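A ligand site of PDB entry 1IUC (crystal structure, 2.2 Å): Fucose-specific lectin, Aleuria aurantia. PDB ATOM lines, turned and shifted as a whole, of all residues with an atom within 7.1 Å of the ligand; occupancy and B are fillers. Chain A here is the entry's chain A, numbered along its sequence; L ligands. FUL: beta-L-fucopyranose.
O3 of the ligand is in hydrogen-bond range of OE1 of Glu 89, 2.5 Å away. NE1 of Trp 153 sits at hydrogen-bond distance from O3 of the ligand (2.8 Å). O4 of the ligand sits at hydrogen-bond distance from NE of Arg 77 (3.0 Å). N of Gln 101 lies within hydrogen-bond range of O2 of the ligand, 3.2 Å away.
The side-chain carboxylate (OE1) of Glu 89 is in hydrogen-bond range of the backbone NH (N) of Gln 101. O of Glu 89 lies within hydrogen-bond range of N of Gly 100, at 2.7 Å. The side-chain carboxylate of Glu 89 is in hydrogen-bond range of the side-chain hydroxyl of Tyr 79 (2.7 Å). NH2 of Arg 77 sits at hydrogen-bond distance from OE1 of Gln 75. The backbone carbonyl oxygen (O) of Ile 130 sits at hydrogen-bond distance from the backbone NH (N) of Trp 149.
CA of Gly 100 touches O2 of the ligand, 3.7 Å away. Leu 102 touches the ligand. Ile 130 touches the ligand (CD1 to C6, 3.8 Å). Trp 149 touches the ligand. Of the 21 residues printed, 8 come within 4 Å of the ligand. The nearest printed residue that does not touch the ligand is Pro 128 (4.1 Å).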
ATOM      1  N   TRP A  68       4.357  18.043  -8.469  1.00  0.00           N
ATOM      2  CA  TRP A  68       4.796  16.877  -9.239  1.00  0.00           C
ATOM      3  C   TRP A  68       3.592  15.955  -9.292  1.00  0.00           C
ATOM      4  O   TRP A  68       2.622  16.146  -8.555  1.00  0.00           O
ATOM      5  CB  TRP A  68       5.996  16.203  -8.574  1.00  0.00           C
ATOM      6  CG  TRP A  68       5.703  15.479  -7.286  1.00  0.00           C
ATOM      7  CD1 TRP A  68       5.372  14.163  -7.139  1.00  0.00           C
ATOM      8  CD2 TRP A  68       5.721  16.035  -5.964  1.00  0.00           C
ATOM      9  NE1 TRP A  68       5.187  13.864  -5.808  1.00  0.00           N
ATOM     10  CE2 TRP A  68       5.389  15.003  -5.069  1.00  0.00           C
ATOM     11  CE3 TRP A  68       5.984  17.323  -5.450  1.00  0.00           C
ATOM     12  CZ2 TRP A  68       5.306  15.201  -3.672  1.00  0.00           C
ATOM     13  CZ3 TRP A  68       5.904  17.520  -4.067  1.00  0.00           C
ATOM     14  CH2 TRP A  68       5.569  16.457  -3.199  1.00  0.00           C
ATOM     15  N   GLN A  75       0.406  16.477  -6.819  1.00  0.00           N
ATOM     16  CA  GLN A  75       0.923  16.869  -5.507  1.00  0.00           C
ATOM     17  C   GLN A  75       1.401  18.327  -5.530  1.00  0.00           C
ATOM     18  O   GLN A  75       2.075  18.755  -6.472  1.00  0.00           O
ATOM     19  CB  GLN A  75       2.113  15.989  -5.102  1.00  0.00           C
ATOM     20  CG  GLN A  75       1.815  14.493  -4.949  1.00  0.00           C
ATOM     21  CD  GLN A  75       0.856  14.213  -3.791  1.00  0.00           C
ATOM     22  OE1 GLN A  75       1.052  14.704  -2.676  1.00  0.00           O
ATOM     23  NE2 GLN A  75      -0.177  13.423  -4.054  1.00  0.00           N
ATOM     24  N   ILE A  76       1.026  19.089  -4.514  1.00  0.00           N
ATOM     25  CA  ILE A  76       1.472  20.476  -4.407  1.00  0.00           C
ATOM     26  C   ILE A  76       1.922  20.728  -2.974  1.00  0.00           C
ATOM     27  O   ILE A  76       1.338  20.219  -2.024  1.00  0.00           O
ATOM     28  CB  ILE A  76       0.333  21.473  -4.726  1.00  0.00           C
ATOM     29  CG1 ILE A  76      -0.187  21.251  -6.145  1.00  0.00           C
ATOM     30  CG2 ILE A  76       0.847  22.922  -4.561  1.00  0.00           C
ATOM     31  CD1 ILE A  76      -1.436  22.030  -6.452  1.00  0.00           C
ATOM     32  N   ARG A  77       2.989  21.509  -2.827  1.00  0.00           N
ATOM     33  CA  ARG A  77       3.493  21.868  -1.508  1.00  0.00           C
ATOM     34  C   ARG A  77       3.683  23.381  -1.524  1.00  0.00           C
ATOM     35  O   ARG A  77       4.311  23.927  -2.441  1.00  0.00           O
ATOM     36  CB  ARG A  77       4.818  21.174  -1.209  1.00  0.00           C
ATOM     37  CG  ARG A  77       4.748  19.653  -1.192  1.00  0.00           C
ATOM     38  CD  ARG A  77       3.930  19.125  -0.009  1.00  0.00           C
ATOM     39  NE  ARG A  77       3.904  17.668   0.017  1.00  0.00           N
ATOM     40  CZ  ARG A  77       3.105  16.900  -0.731  1.00  0.00           C
ATOM     41  NH1 ARG A  77       2.251  17.469  -1.576  1.00  0.00           N
ATOM     42  NH2 ARG A  77       3.162  15.581  -0.636  1.00  0.00           N
ATOM     43  N   TYR A  79       5.032  26.597   0.758  1.00  0.00           N
ATOM     44  CA  TYR A  79       5.787  26.976   1.933  1.00  0.00           C
ATOM     45  C   TYR A  79       5.544  28.439   2.311  1.00  0.00           C
ATOM     46  O   TYR A  79       5.385  29.306   1.447  1.00  0.00           O
ATOM     47  CB  TYR A  79       7.284  26.725   1.695  1.00  0.00           C
ATOM     48  CG  TYR A  79       7.547  25.252   1.415  1.00  0.00           C
ATOM     49  CD1 TYR A  79       7.600  24.777   0.093  1.00  0.00           C
ATOM     50  CD2 TYR A  79       7.573  24.332   2.461  1.00  0.00           C
ATOM     51  CE1 TYR A  79       7.677  23.400  -0.171  1.00  0.00           C
ATOM     52  CE2 TYR A  79       7.639  22.962   2.209  1.00  0.00           C
ATOM     53  CZ  TYR A  79       7.690  22.505   0.899  1.00  0.00           C
ATOM     54  OH  TYR A  79       7.687  21.148   0.662  1.00  0.00           O
ATOM     55  N   GLU A  89       4.245  24.402   6.092  1.00  0.00           N
ATOM     56  CA  GLU A  89       3.950  23.817   4.794  1.00  0.00           C
ATOM     57  C   GLU A  89       2.515  23.351   4.611  1.00  0.00           C
ATOM     58  O   GLU A  89       1.966  22.673   5.488  1.00  0.00           O
ATOM     59  CB  GLU A  89       4.885  22.619   4.579  1.00  0.00           C
ATOM     60  CG  GLU A  89       4.543  21.714   3.399  1.00  0.00           C
ATOM     61  CD  GLU A  89       5.310  20.388   3.446  1.00  0.00           C
ATOM     62  OE1 GLU A  89       5.164  19.652   4.452  1.00  0.00           O
ATOM     63  OE2 GLU A  89       6.066  20.090   2.498  1.00  0.00           O
ATOM     64  N   PHE A  90       1.910  23.722   3.496  1.00  0.00           N
ATOM     65  CA  PHE A  90       0.554  23.275   3.196  1.00  0.00           C
ATOM     66  C   PHE A  90       0.682  22.214   2.108  1.00  0.00           C
ATOM     67  O   PHE A  90       1.505  22.353   1.195  1.00  0.00           O
ATOM     68  CB  PHE A  90      -0.333  24.427   2.767  1.00  0.00           C
ATOM     69  CG  PHE A  90      -0.651  25.377   3.901  1.00  0.00           C
ATOM     70  CD1 PHE A  90      -0.194  26.685   3.879  1.00  0.00           C
ATOM     71  CD2 PHE A  90      -1.340  24.917   5.016  1.00  0.00           C
ATOM     72  CE1 PHE A  90      -0.410  27.531   4.954  1.00  0.00           C
ATOM     73  CE2 PHE A  90      -1.564  25.759   6.111  1.00  0.00           C
ATOM     74  CZ  PHE A  90      -1.091  27.065   6.071  1.00  0.00           C
ATOM     75  N   VAL A  91      -0.121  21.173   2.225  1.00  0.00           N
ATOM     76  CA  VAL A  91      -0.044  20.045   1.299  1.00  0.00           C
ATOM     77  C   VAL A  91      -1.325  19.776   0.552  1.00  0.00           C
ATOM     78  O   VAL A  91      -2.409  19.743   1.141  1.00  0.00           O
ATOM     79  CB  VAL A  91       0.296  18.742   2.087  1.00  0.00           C
ATOM     80  CG1 VAL A  91       0.266  17.535   1.162  1.00  0.00           C
ATOM     81  CG2 VAL A  91       1.664  18.867   2.776  1.00  0.00           C
ATOM     82  N   ASP A  93      -2.719  16.816  -1.355  1.00  0.00           N
ATOM     83  CA  ASP A  93      -2.388  15.403  -1.533  1.00  0.00           C
ATOM     84  C   ASP A  93      -2.963  14.699  -2.758  1.00  0.00           C
ATOM     85  O   ASP A  93      -2.926  13.471  -2.832  1.00  0.00           O
ATOM     86  CB  ASP A  93      -2.787  14.601  -0.301  1.00  0.00           C
ATOM     87  CG  ASP A  93      -4.296  14.566  -0.085  1.00  0.00           C
ATOM     88  OD1 ASP A  93      -5.064  14.854  -1.036  1.00  0.00           O
ATOM     89  OD2 ASP A  93      -4.716  14.219   1.034  1.00  0.00           O
ATOM     90  N   ILE A  98      -4.196  19.869   3.139  1.00  0.00           N
ATOM     91  CA  ILE A  98      -3.939  19.618   4.548  1.00  0.00           C
ATOM     92  C   ILE A  98      -2.647  20.312   4.961  1.00  0.00           C
ATOM     93  O   ILE A  98      -2.024  21.012   4.160  1.00  0.00           O
ATOM     94  CB  ILE A  98      -3.803  18.111   4.847  1.00  0.00           C
ATOM     95  CG1 ILE A  98      -2.687  17.509   3.997  1.00  0.00           C
ATOM     96  CG2 ILE A  98      -5.122  17.402   4.553  1.00  0.00           C
ATOM     97  CD1 ILE A  98      -2.403  16.053   4.304  1.00  0.00           C
ATOM     98  N   THR A  99      -2.244  20.104   6.205  1.00  0.00           N
ATOM     99  CA  THR A  99      -1.027  20.709   6.712  1.00  0.00           C
ATOM    100  C   THR A  99       0.118  19.709   6.686  1.00  0.00           C
ATOM    101  O   THR A  99      -0.054  18.554   7.072  1.00  0.00           O
ATOM    102  CB  THR A  99      -1.255  21.217   8.129  1.00  0.00           C
ATOM    103  OG1 THR A  99      -2.326  22.167   8.115  1.00  0.00           O
ATOM    104  CG2 THR A  99       0.000  21.860   8.697  1.00  0.00           C
ATOM    105  N   GLY A 100       1.274  20.161   6.213  1.00  0.00           N
ATOM    106  CA  GLY A 100       2.436  19.290   6.136  1.00  0.00           C
ATOM    107  C   GLY A 100       3.166  19.124   7.452  1.00  0.00           C
ATOM    108  O   GLY A 100       2.889  19.819   8.434  1.00  0.00           O
ATOM    109  N   GLN A 101       4.131  18.216   7.458  1.00  0.00           N
ATOM    110  CA  GLN A 101       4.909  17.918   8.649  1.00  0.00           C
ATOM    111  C   GLN A 101       6.048  18.883   8.939  1.00  0.00           C
ATOM    112  O   GLN A 101       6.555  18.919  10.068  1.00  0.00           O
ATOM    113  CB  GLN A 101       5.465  16.496   8.556  1.00  0.00           C
ATOM    114  CG  GLN A 101       4.370  15.461   8.338  1.00  0.00           C
ATOM    115  CD  GLN A 101       3.316  15.486   9.447  1.00  0.00           C
ATOM    116  OE1 GLN A 101       3.570  15.050  10.575  1.00  0.00           O
ATOM    117  NE2 GLN A 101       2.130  16.003   9.137  1.00  0.00           N
ATOM    118  N   LEU A 102       6.446  19.681   7.960  1.00  0.00           N
ATOM    119  CA  LEU A 102       7.558  20.610   8.154  1.00  0.00           C
ATOM    120  C   LEU A 102       7.424  21.556   9.344  1.00  0.00           C
ATOM    121  O   LEU A 102       8.414  21.853  10.028  1.00  0.00           O
ATOM    122  CB  LEU A 102       7.791  21.427   6.876  1.00  0.00           C
ATOM    123  CG  LEU A 102       8.929  22.458   6.901  1.00  0.00           C
ATOM    124  CD1 LEU A 102      10.245  21.809   7.317  1.00  0.00           C
ATOM    125  CD2 LEU A 102       9.057  23.095   5.517  1.00  0.00           C
ATOM    126  N   GLY A 103       6.216  22.043   9.609  1.00  0.00           N
ATOM    127  CA  GLY A 103       6.033  22.950  10.728  1.00  0.00           C
ATOM    128  C   GLY A 103       6.505  22.377  12.058  1.00  0.00           C
ATOM    129  O   GLY A 103       7.105  23.083  12.869  1.00  0.00           O
ATOM    130  N   PRO A 128       9.445  12.247  -4.289  1.00  0.00           N
ATOM    131  CA  PRO A 128      10.091  13.508  -4.661  1.00  0.00           C
ATOM    132  C   PRO A 128      11.294  13.845  -3.804  1.00  0.00           C
ATOM    133  O   PRO A 128      11.488  13.290  -2.728  1.00  0.00           O
ATOM    134  CB  PRO A 128       8.969  14.519  -4.488  1.00  0.00           C
ATOM    135  CG  PRO A 128       8.269  13.992  -3.268  1.00  0.00           C
ATOM    136  CD  PRO A 128       8.187  12.504  -3.567  1.00  0.00           C
ATOM    137  N   ASN A 129      12.106  14.768  -4.306  1.00  0.00           N
ATOM    138  CA  ASN A 129      13.265  15.274  -3.593  1.00  0.00           C
ATOM    139  C   ASN A 129      12.979  16.765  -3.528  1.00  0.00           C
ATOM    140  O   ASN A 129      13.006  17.448  -4.566  1.00  0.00           O
ATOM    141  CB  ASN A 129      14.552  15.017  -4.381  1.00  0.00           C
ATOM    142  CG  ASN A 129      14.880  13.541  -4.476  1.00  0.00           C
ATOM    143  OD1 ASN A 129      15.447  12.963  -3.553  1.00  0.00           O
ATOM    144  ND2 ASN A 129      14.502  12.918  -5.598  1.00  0.00           N
ATOM    145  N   ILE A 130      12.701  17.268  -2.336  1.00  0.00           N
ATOM    146  CA  ILE A 130      12.383  18.681  -2.162  1.00  0.00           C
ATOM    147  C   ILE A 130      13.481  19.428  -1.415  1.00  0.00           C
ATOM    148  O   ILE A 130      14.105  18.897  -0.486  1.00  0.00           O
ATOM    149  CB  ILE A 130      11.063  18.857  -1.374  1.00  0.00           C
ATOM    150  CG1 ILE A 130       9.936  18.049  -2.027  1.00  0.00           C
ATOM    151  CG2 ILE A 130      10.663  20.336  -1.336  1.00  0.00           C
ATOM    152  CD1 ILE A 130       8.681  17.986  -1.179  1.00  0.00           C
ATOM    153  N   TRP A 149      14.239  17.325   2.017  1.00  0.00           N
ATOM    154  CA  TRP A 149      13.281  16.266   2.251  1.00  0.00           C
ATOM    155  C   TRP A 149      13.556  15.122   1.291  1.00  0.00           C
ATOM    156  O   TRP A 149      13.430  15.271   0.073  1.00  0.00           O
ATOM    157  CB  TRP A 149      11.831  16.696   2.051  1.00  0.00           C
ATOM    158  CG  TRP A 149      10.900  15.670   2.633  1.00  0.00           C
ATOM    159  CD1 TRP A 149      10.439  15.604   3.924  1.00  0.00           C
ATOM    160  CD2 TRP A 149      10.378  14.512   1.967  1.00  0.00           C
ATOM    161  NE1 TRP A 149       9.660  14.491   4.094  1.00  0.00           N
ATOM    162  CE2 TRP A 149       9.599  13.803   2.920  1.00  0.00           C
ATOM    163  CE3 TRP A 149      10.474  14.015   0.662  1.00  0.00           C
ATOM    164  CZ2 TRP A 149       8.934  12.616   2.598  1.00  0.00           C
ATOM    165  CZ3 TRP A 149       9.812  12.834   0.347  1.00  0.00           C
ATOM    166  CH2 TRP A 149       9.047  12.148   1.315  1.00  0.00           C
ATOM    167  N   GLY A 151      12.505  11.633   2.360  1.00  0.00           N
ATOM    168  CA  GLY A 151      11.983  10.615   3.248  1.00  0.00           C
ATOM    169  C   GLY A 151      11.630  11.268   4.573  1.00  0.00           C
ATOM    170  O   GLY A 151      10.674  10.880   5.244  1.00  0.00           O
ATOM    171  N   TRP A 153      12.514  15.334   6.845  1.00  0.00           N
ATOM    172  CA  TRP A 153      13.137  16.648   6.781  1.00  0.00           C
ATOM    173  C   TRP A 153      14.433  16.706   7.570  1.00  0.00           C
ATOM    174  O   TRP A 153      14.492  16.244   8.700  1.00  0.00           O
ATOM    175  CB  TRP A 153      12.182  17.732   7.311  1.00  0.00           C
ATOM    176  CG  TRP A 153      11.030  18.046   6.417  1.00  0.00           C
ATOM    177  CD1 TRP A 153       9.729  17.650   6.564  1.00  0.00           C
ATOM    178  CD2 TRP A 153      11.083  18.788   5.191  1.00  0.00           C
ATOM    179  NE1 TRP A 153       8.960  18.109   5.505  1.00  0.00           N
ATOM    180  CE2 TRP A 153       9.771  18.807   4.646  1.00  0.00           C
ATOM    181  CE3 TRP A 153      12.114  19.445   4.491  1.00  0.00           C
ATOM    182  CZ2 TRP A 153       9.471  19.453   3.450  1.00  0.00           C
ATOM    183  CZ3 TRP A 153      11.805  20.079   3.294  1.00  0.00           C
ATOM    184  CH2 TRP A 153      10.494  20.078   2.794  1.00  0.00           C
HETATM  185  C1  FUL L   1       4.265  14.861   3.044  1.00  0.00           C
HETATM  186  C2  FUL L   1       4.546  16.121   3.867  1.00  0.00           C
HETATM  187  O2  FUL L   1       3.922  16.032   5.144  1.00  0.00           O
HETATM  188  C3  FUL L   1       6.062  16.279   4.039  1.00  0.00           C
HETATM  189  O3  FUL L   1       6.340  17.459   4.795  1.00  0.00           O
HETATM  190  C4  FUL L   1       6.707  16.342   2.652  1.00  0.00           C
HETATM  191  O4  FUL L   1       6.192  17.462   1.940  1.00  0.00           O
HETATM  192  C5  FUL L   1       6.361  15.063   1.884  1.00  0.00           C
HETATM  193  C6  FUL L   1       6.927  15.044   0.475  1.00  0.00           C
HETATM  194  O5  FUL L   1       4.926  14.932   1.768  1.00  0.00           O
HETATM  195  O1  FUL L   1       2.914  14.771   2.803  1.00  0.00           O
